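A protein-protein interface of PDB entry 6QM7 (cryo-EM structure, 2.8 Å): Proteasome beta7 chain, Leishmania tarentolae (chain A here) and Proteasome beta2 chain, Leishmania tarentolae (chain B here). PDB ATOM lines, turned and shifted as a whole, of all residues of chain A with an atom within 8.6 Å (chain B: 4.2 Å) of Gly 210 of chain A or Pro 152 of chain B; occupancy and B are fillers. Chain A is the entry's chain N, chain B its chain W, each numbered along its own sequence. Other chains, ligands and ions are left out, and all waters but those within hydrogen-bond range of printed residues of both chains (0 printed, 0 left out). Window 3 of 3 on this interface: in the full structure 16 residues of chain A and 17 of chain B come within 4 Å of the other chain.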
ATOM      1  N   ARG A 176     -13.983 -15.958  24.482  1.00  0.00           N
ATOM      2  CA  ARG A 176     -14.115 -15.857  25.965  1.00  0.00           C
ATOM      3  C   ARG A 176     -14.065 -14.421  26.488  1.00  0.00           C
ATOM      4  O   ARG A 176     -14.702 -14.169  27.504  1.00  0.00           O
ATOM      5  CB  ARG A 176     -13.056 -16.744  26.624  1.00  0.00           C
ATOM      6  CG  ARG A 176     -13.259 -18.225  26.334  1.00  0.00           C
ATOM      7  CD  ARG A 176     -14.463 -18.741  27.080  1.00  0.00           C
ATOM      8  NE  ARG A 176     -14.998 -19.981  26.559  1.00  0.00           N
ATOM      9  CZ  ARG A 176     -15.935 -20.696  27.172  1.00  0.00           C
ATOM     10  NH1 ARG A 176     -16.446 -20.303  28.329  1.00  0.00           N
ATOM     11  NH2 ARG A 176     -16.368 -21.812  26.619  1.00  0.00           N
ATOM     12  N   TRP A 206     -17.716 -23.656  16.190  1.00  0.00           N
ATOM     13  CA  TRP A 206     -18.997 -23.419  16.904  1.00  0.00           C
ATOM     14  C   TRP A 206     -19.911 -24.648  16.842  1.00  0.00           C
ATOM     15  O   TRP A 206     -20.990 -24.595  17.456  1.00  0.00           O
ATOM     16  CB  TRP A 206     -19.679 -22.213  16.263  1.00  0.00           C
ATOM     17  CG  TRP A 206     -18.957 -20.944  16.551  1.00  0.00           C
ATOM     18  CD1 TRP A 206     -18.023 -20.293  15.794  1.00  0.00           C
ATOM     19  CD2 TRP A 206     -19.104 -20.190  17.750  1.00  0.00           C
ATOM     20  NE1 TRP A 206     -17.587 -19.170  16.446  1.00  0.00           N
ATOM     21  CE2 TRP A 206     -18.222 -19.095  17.652  1.00  0.00           C
ATOM     22  CE3 TRP A 206     -19.898 -20.350  18.893  1.00  0.00           C
ATOM     23  CZ2 TRP A 206     -18.122 -18.154  18.670  1.00  0.00           C
ATOM     24  CZ3 TRP A 206     -19.805 -19.414  19.892  1.00  0.00           C
ATOM     25  CH2 TRP A 206     -18.918 -18.340  19.784  1.00  0.00           C
ATOM     26  N   GLU A 207     -19.509 -25.700  16.126  1.00  0.00           N
ATOM     27  CA  GLU A 207     -20.387 -26.834  15.754  1.00  0.00           C
ATOM     28  C   GLU A 207     -19.883 -28.094  16.459  1.00  0.00           C
ATOM     29  O   GLU A 207     -19.818 -29.157  15.807  1.00  0.00           O
ATOM     30  CB  GLU A 207     -20.438 -26.962  14.230  1.00  0.00           C
ATOM     31  CG  GLU A 207     -21.378 -25.961  13.571  1.00  0.00           C
ATOM     32  CD  GLU A 207     -20.913 -25.464  12.209  1.00  0.00           C
ATOM     33  OE1 GLU A 207     -19.971 -24.625  12.174  1.00  0.00           O
ATOM     34  OE2 GLU A 207     -21.490 -25.908  11.185  1.00  0.00           O
ATOM     35  N   TYR A 208     -19.570 -27.986  17.753  1.00  0.00           N
ATOM     36  CA  TYR A 208     -19.422 -29.153  18.657  1.00  0.00           C
ATOM     37  C   TYR A 208     -20.804 -29.784  18.810  1.00  0.00           C
ATOM     38  O   TYR A 208     -21.765 -29.019  18.872  1.00  0.00           O
ATOM     39  CB  TYR A 208     -18.858 -28.753  20.020  1.00  0.00           C
ATOM     40  CG  TYR A 208     -17.476 -28.159  19.987  1.00  0.00           C
ATOM     41  CD1 TYR A 208     -16.388 -28.885  19.536  1.00  0.00           C
ATOM     42  CD2 TYR A 208     -17.249 -26.867  20.432  1.00  0.00           C
ATOM     43  CE1 TYR A 208     -15.112 -28.337  19.515  1.00  0.00           C
ATOM     44  CE2 TYR A 208     -15.985 -26.302  20.411  1.00  0.00           C
ATOM     45  CZ  TYR A 208     -14.908 -27.036  19.951  1.00  0.00           C
ATOM     46  OH  TYR A 208     -13.670 -26.455  19.940  1.00  0.00           O
ATOM     47  N   GLU A 209     -20.900 -31.115  18.864  1.00  0.00           N
ATOM     48  CA  GLU A 209     -22.199 -31.825  19.042  1.00  0.00           C
ATOM     49  C   GLU A 209     -22.806 -31.437  20.398  1.00  0.00           C
ATOM     50  O   GLU A 209     -24.029 -31.566  20.541  1.00  0.00           O
ATOM     51  CB  GLU A 209     -22.056 -33.344  18.880  1.00  0.00           C
ATOM     52  CG  GLU A 209     -21.652 -34.098  20.149  1.00  0.00           C
ATOM     53  CD  GLU A 209     -21.061 -35.492  19.933  1.00  0.00           C
ATOM     54  OE1 GLU A 209     -19.941 -35.595  19.360  1.00  0.00           O
ATOM     55  OE2 GLU A 209     -21.717 -36.486  20.337  1.00  0.00           O
ATOM     56  N   GLY A 210     -21.993 -30.973  21.348  1.00  0.00           N
ATOM     57  CA  GLY A 210     -22.440 -30.602  22.702  1.00  0.00           C
ATOM     58  C   GLY A 210     -23.000 -29.196  22.806  1.00  0.00           C
ATOM     59  O   GLY A 210     -23.422 -28.834  23.918  1.00  0.00           O
ATOM     60  N   TYR A 211     -22.961 -28.427  21.721  1.00  0.00           N
ATOM     61  CA  TYR A 211     -23.506 -27.050  21.602  1.00  0.00           C
ATOM     62  C   TYR A 211     -24.844 -27.082  20.882  1.00  0.00           C
ATOM     63  O   TYR A 211     -25.451 -26.013  20.734  1.00  0.00           O
ATOM     64  CB  TYR A 211     -22.556 -26.154  20.800  1.00  0.00           C
ATOM     65  CG  TYR A 211     -21.337 -25.656  21.524  1.00  0.00           C
ATOM     66  CD1 TYR A 211     -20.486 -24.766  20.908  1.00  0.00           C
ATOM     67  CD2 TYR A 211     -21.050 -26.030  22.823  1.00  0.00           C
ATOM     68  CE1 TYR A 211     -19.362 -24.274  21.553  1.00  0.00           C
ATOM     69  CE2 TYR A 211     -19.932 -25.554  23.479  1.00  0.00           C
ATOM     70  CZ  TYR A 211     -19.078 -24.671  22.848  1.00  0.00           C
ATOM     71  OH  TYR A 211     -17.980 -24.193  23.519  1.00  0.00           O
ATOM     72  N   CYS A 212     -25.282 -28.259  20.437  1.00  0.00           N
ATOM     73  CA  CYS A 212     -26.579 -28.442  19.736  1.00  0.00           C
ATOM     74  C   CYS A 212     -27.735 -28.027  20.663  1.00  0.00           C
ATOM     75  O   CYS A 212     -27.579 -28.058  21.895  1.00  0.00           O
ATOM     76  CB  CYS A 212     -26.756 -29.876  19.265  1.00  0.00           C
ATOM     77  SG  CYS A 212     -27.312 -30.978  20.593  1.00  0.00           S
ATOM     78  N   PHE A 213     -28.850 -27.623  20.067  1.00  0.00           N
ATOM     79  CA  PHE A 213     -30.045 -27.085  20.759  1.00  0.00           C
ATOM     80  C   PHE A 213     -30.564 -28.081  21.792  1.00  0.00           C
ATOM     81  O   PHE A 213     -30.969 -27.641  22.867  1.00  0.00           O
ATOM     82  CB  PHE A 213     -31.149 -26.804  19.739  1.00  0.00           C
ATOM     83  CG  PHE A 213     -32.273 -25.952  20.255  1.00  0.00           C
ATOM     84  CD1 PHE A 213     -32.289 -24.591  20.009  1.00  0.00           C
ATOM     85  CD2 PHE A 213     -33.315 -26.516  20.976  1.00  0.00           C
ATOM     86  CE1 PHE A 213     -33.328 -23.809  20.479  1.00  0.00           C
ATOM     87  CE2 PHE A 213     -34.351 -25.727  21.456  1.00  0.00           C
ATOM     88  CZ  PHE A 213     -34.360 -24.374  21.201  1.00  0.00           C
ATOM     89  N   GLU A 214     -30.587 -29.372  21.441  1.00  0.00           N
ATOM     90  CA  GLU A 214     -31.215 -30.456  22.239  1.00  0.00           C
ATOM     91  C   GLU A 214     -30.423 -30.678  23.533  1.00  0.00           C
ATOM     92  O   GLU A 214     -31.071 -30.812  24.579  1.00  0.00           O
ATOM     93  CB  GLU A 214     -31.308 -31.742  21.423  1.00  0.00           C
ATOM     94  CG  GLU A 214     -32.323 -32.727  21.980  1.00  0.00           C
ATOM     95  CD  GLU A 214     -32.303 -34.123  21.364  1.00  0.00           C
ATOM     96  OE1 GLU A 214     -32.556 -34.240  20.143  1.00  0.00           O
ATOM     97  OE2 GLU A 214     -32.034 -35.098  22.109  1.00  0.00           O
ATOM     98  N   LYS A 215     -29.089 -30.713  23.475  1.00  0.00           N
ATOM     99  CA  LYS A 215     -28.221 -30.964  24.660  1.00  0.00           C
ATOM    100  C   LYS A 215     -28.281 -29.770  25.612  1.00  0.00           C
ATOM    101  O   LYS A 215     -28.570 -29.991  26.805  1.00  0.00           O
ATOM    102  CB  LYS A 215     -26.767 -31.232  24.258  1.00  0.00           C
ATOM    103  CG  LYS A 215     -26.546 -32.532  23.499  1.00  0.00           C
ATOM    104  CD  LYS A 215     -26.510 -33.783  24.372  1.00  0.00           C
ATOM    105  CE  LYS A 215     -25.136 -34.418  24.442  1.00  0.00           C
ATOM    106  NZ  LYS A 215     -24.607 -34.735  23.093  1.00  0.00           N
ATOM    107  N   THR A 216     -28.034 -28.565  25.096  1.00  0.00           N
ATOM    108  CA  THR A 216     -27.892 -27.311  25.880  1.00  0.00           C
ATOM    109  C   THR A 216     -29.235 -26.829  26.435  1.00  0.00           C
ATOM    110  O   THR A 216     -29.220 -25.886  27.248  1.00  0.00           O
ATOM    111  CB  THR A 216     -27.269 -26.185  25.046  1.00  0.00           C
ATOM    112  OG1 THR A 216     -28.035 -26.027  23.853  1.00  0.00           O
ATOM    113  CG2 THR A 216     -25.824 -26.459  24.698  1.00  0.00           C
ATOM    114  N   ALA A 217     -30.347 -27.410  25.992  1.00  0.00           N
ATOM    115  CA  ALA A 217     -31.702 -27.123  26.506  1.00  0.00           C
ATOM    116  C   ALA A 217     -31.743 -27.332  28.022  1.00  0.00           C
ATOM    117  O   ALA A 217     -31.156 -28.308  28.496  1.00  0.00           O
ATOM    118  CB  ALA A 217     -32.700 -28.003  25.811  1.00  0.00           C
ATOM    119  N   VAL B  35     -14.235 -32.636  30.723  1.00  0.00           N
ATOM    120  CA  VAL B  35     -14.462 -32.782  29.264  1.00  0.00           C
ATOM    121  C   VAL B  35     -15.301 -34.033  29.077  1.00  0.00           C
ATOM    122  O   VAL B  35     -15.118 -34.977  29.825  1.00  0.00           O
ATOM    123  CB  VAL B  35     -13.148 -32.840  28.460  1.00  0.00           C
ATOM    124  CG1 VAL B  35     -12.233 -31.660  28.764  1.00  0.00           C
ATOM    125  CG2 VAL B  35     -12.403 -34.142  28.682  1.00  0.00           C
ATOM    126  N   VAL B  36     -16.211 -33.987  28.123  1.00  0.00           N
ATOM    127  CA  VAL B  36     -16.870 -35.171  27.514  1.00  0.00           C
ATOM    128  C   VAL B  36     -15.920 -35.708  26.451  1.00  0.00           C
ATOM    129  O   VAL B  36     -15.516 -34.923  25.591  1.00  0.00           O
ATOM    130  CB  VAL B  36     -18.226 -34.768  26.922  1.00  0.00           C
ATOM    131  CG1 VAL B  36     -18.774 -35.813  25.989  1.00  0.00           C
ATOM    132  CG2 VAL B  36     -19.224 -34.466  28.014  1.00  0.00           C
ATOM    133  N   LEU B 139     -22.003 -33.802  31.389  1.00  0.00           N
ATOM    134  CA  LEU B 139     -21.090 -32.901  32.095  1.00  0.00           C
ATOM    135  C   LEU B 139     -21.800 -31.569  32.240  1.00  0.00           C
ATOM    136  O   LEU B 139     -22.353 -31.109  31.252  1.00  0.00           O
ATOM    137  CB  LEU B 139     -19.834 -32.771  31.249  1.00  0.00           C
ATOM    138  CG  LEU B 139     -18.824 -31.805  31.833  1.00  0.00           C
ATOM    139  CD1 LEU B 139     -18.204 -32.379  33.100  1.00  0.00           C
ATOM    140  CD2 LEU B 139     -17.768 -31.473  30.799  1.00  0.00           C
ATOM    141  N   LEU B 151     -22.539 -28.745  29.115  1.00  0.00           N
ATOM    142  CA  LEU B 151     -21.577 -28.454  28.026  1.00  0.00           C
ATOM    143  C   LEU B 151     -20.615 -29.603  27.844  1.00  0.00           C
ATOM    144  O   LEU B 151     -20.430 -30.404  28.750  1.00  0.00           O
ATOM    145  CB  LEU B 151     -20.799 -27.202  28.410  1.00  0.00           C
ATOM    146  CG  LEU B 151     -21.587 -25.906  28.334  1.00  0.00           C
ATOM    147  CD1 LEU B 151     -20.779 -24.756  28.917  1.00  0.00           C
ATOM    148  CD2 LEU B 151     -21.998 -25.633  26.892  1.00  0.00           C
ATOM    149  N   PRO B 152     -19.945 -29.680  26.683  1.00  0.00           N
ATOM    150  CA  PRO B 152     -18.973 -30.731  26.420  1.00  0.00           C
ATOM    151  C   PRO B 152     -17.619 -30.511  27.100  1.00  0.00           C
ATOM    152  O   PRO B 152     -16.906 -31.454  27.191  1.00  0.00           O
ATOM    153  CB  PRO B 152     -18.846 -30.657  24.903  1.00  0.00           C
ATOM    154  CG  PRO B 152     -18.975 -29.194  24.626  1.00  0.00           C
ATOM    155  CD  PRO B 152     -20.098 -28.772  25.546  1.00  0.00           C
ATOM    156  N   PHE B 153     -17.289 -29.292  27.523  1.00  0.00           N
ATOM    157  CA  PHE B 153     -16.105 -29.000  28.376  1.00  0.00           C
ATOM    158  C   PHE B 153     -16.387 -27.771  29.238  1.00  0.00           C
ATOM    159  O   PHE B 153     -16.882 -26.757  28.726  1.00  0.00           O
ATOM    160  CB  PHE B 153     -14.826 -28.815  27.553  1.00  0.00           C
ATOM    161  CG  PHE B 153     -14.915 -27.746  26.502  1.00  0.00           C
ATOM    162  CD1 PHE B 153     -14.431 -26.477  26.741  1.00  0.00           C
ATOM    163  CD2 PHE B 153     -15.521 -27.994  25.282  1.00  0.00           C
ATOM    164  CE1 PHE B 153     -14.526 -25.484  25.776  1.00  0.00           C
ATOM    165  CE2 PHE B 153     -15.612 -27.005  24.311  1.00  0.00           C
ATOM    166  CZ  PHE B 153     -15.122 -25.744  24.565  1.00  0.00           C
ATOM    167  N   TYR B 171      -9.659 -28.818  22.713  1.00  0.00           N
ATOM    168  CA  TYR B 171     -10.826 -29.735  22.742  1.00  0.00           C
ATOM    169  C   TYR B 171     -11.245 -30.027  21.309  1.00  0.00           C
ATOM    170  O   TYR B 171     -11.343 -29.094  20.512  1.00  0.00           O
ATOM    171  CB  TYR B 171     -12.034 -29.168  23.486  1.00  0.00           C
ATOM    172  CG  TYR B 171     -13.205 -30.113  23.555  1.00  0.00           C
ATOM    173  CD1 TYR B 171     -13.255 -31.111  24.511  1.00  0.00           C
ATOM    174  CD2 TYR B 171     -14.269 -30.024  22.670  1.00  0.00           C
ATOM    175  CE1 TYR B 171     -14.332 -31.984  24.602  1.00  0.00           C
ATOM    176  CE2 TYR B 171     -15.349 -30.892  22.739  1.00  0.00           C
ATOM    177  CZ  TYR B 171     -15.390 -31.876  23.714  1.00  0.00           C
ATOM    178  OH  TYR B 171     -16.441 -32.752  23.797  1.00  0.00           O
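The side-chain hydroxyl of Tyr 171 of chain B sits at hydrogen-bond distance from the backbone carbonyl oxygen of Val 36 of chain B (3.0 Å). The backbone carbonyl oxygen (O) of Pro 152 of chain B lies within hydrogen-bond range of the backbone NH (N) of Val 36 of chain B (2.8 Å). The backbone carbonyl oxygen (O) of Leu 139 of chain B is in hydrogen-bond range of the backbone NH (N) of Leu 151 of chain B (3.2 Å).
Tyr 208 of chain A touches Phe 153 of chain B. Tyr 208 of chain A touches Tyr 171 of chain B. Pro 152 of chain B touches Gly 210 of chain A. CE2 of Tyr 211 of chain A touches CD2 of Leu 151 of chain B (3.99 Å). CD of Pro 152 of chain B touches CE2 of Tyr 211 of chain A, 3.8 Å away. Tyr 211 of chain A touches Phe 153 of chain B (OH to CZ, 3.4 Å).
Of chain B, only Pro 152 comes within 4 Å of Gly 210 of chain A. Of chain A, only Gly 210 (3.7 Å) and Tyr 211 (3.8 Å) come within 4 Å of Pro 152 of chain B. Of the printed residues of chain B, Tyr 208 of chain A touches Phe 153 (3.98 Å) and Tyr 171 (3.6 Å). Of the printed residues of chain B, Tyr 211 of chain A touches Leu 151 (3.99 Å), Pro 152 (3.8 Å) and Phe 153 (3.4 Å). Of the printed residues of chain A, Tyr 171 of chain B touches Tyr 208 (3.6 Å). Of the printed residues of chain A, Phe 153 of chain B touches Tyr 208 (3.98 Å) and Tyr 211 (3.4 Å). Of the printed residues of chain A, Leu 151 of chain B touches Tyr 211. Val 36 of chain B touches none of the printed residues of chain A. The nearest residue of chain A that does not touch Pro 152 of chain B is Tyr 208 of chain A (4.6 Å). The nearest printed residue of chain A that does not touch Tyr 171 of chain B is Gly 210 of chain A (6.3 Å).
Hydrophobic or aromatic side chains of chain B within 4 Å of the printed part of chain A: Leu 151, Pro 152, Phe 153 and Tyr 171. Of the 13 printed residues of chain A, 3 touch a printed residue of chain B. Among the printed residues, 6 pairs touch across the chains. Among the printed residues, no Asp or Glu carboxylate lies within 4 Å of a Lys or Arg side-chain nitrogen of the other chain.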
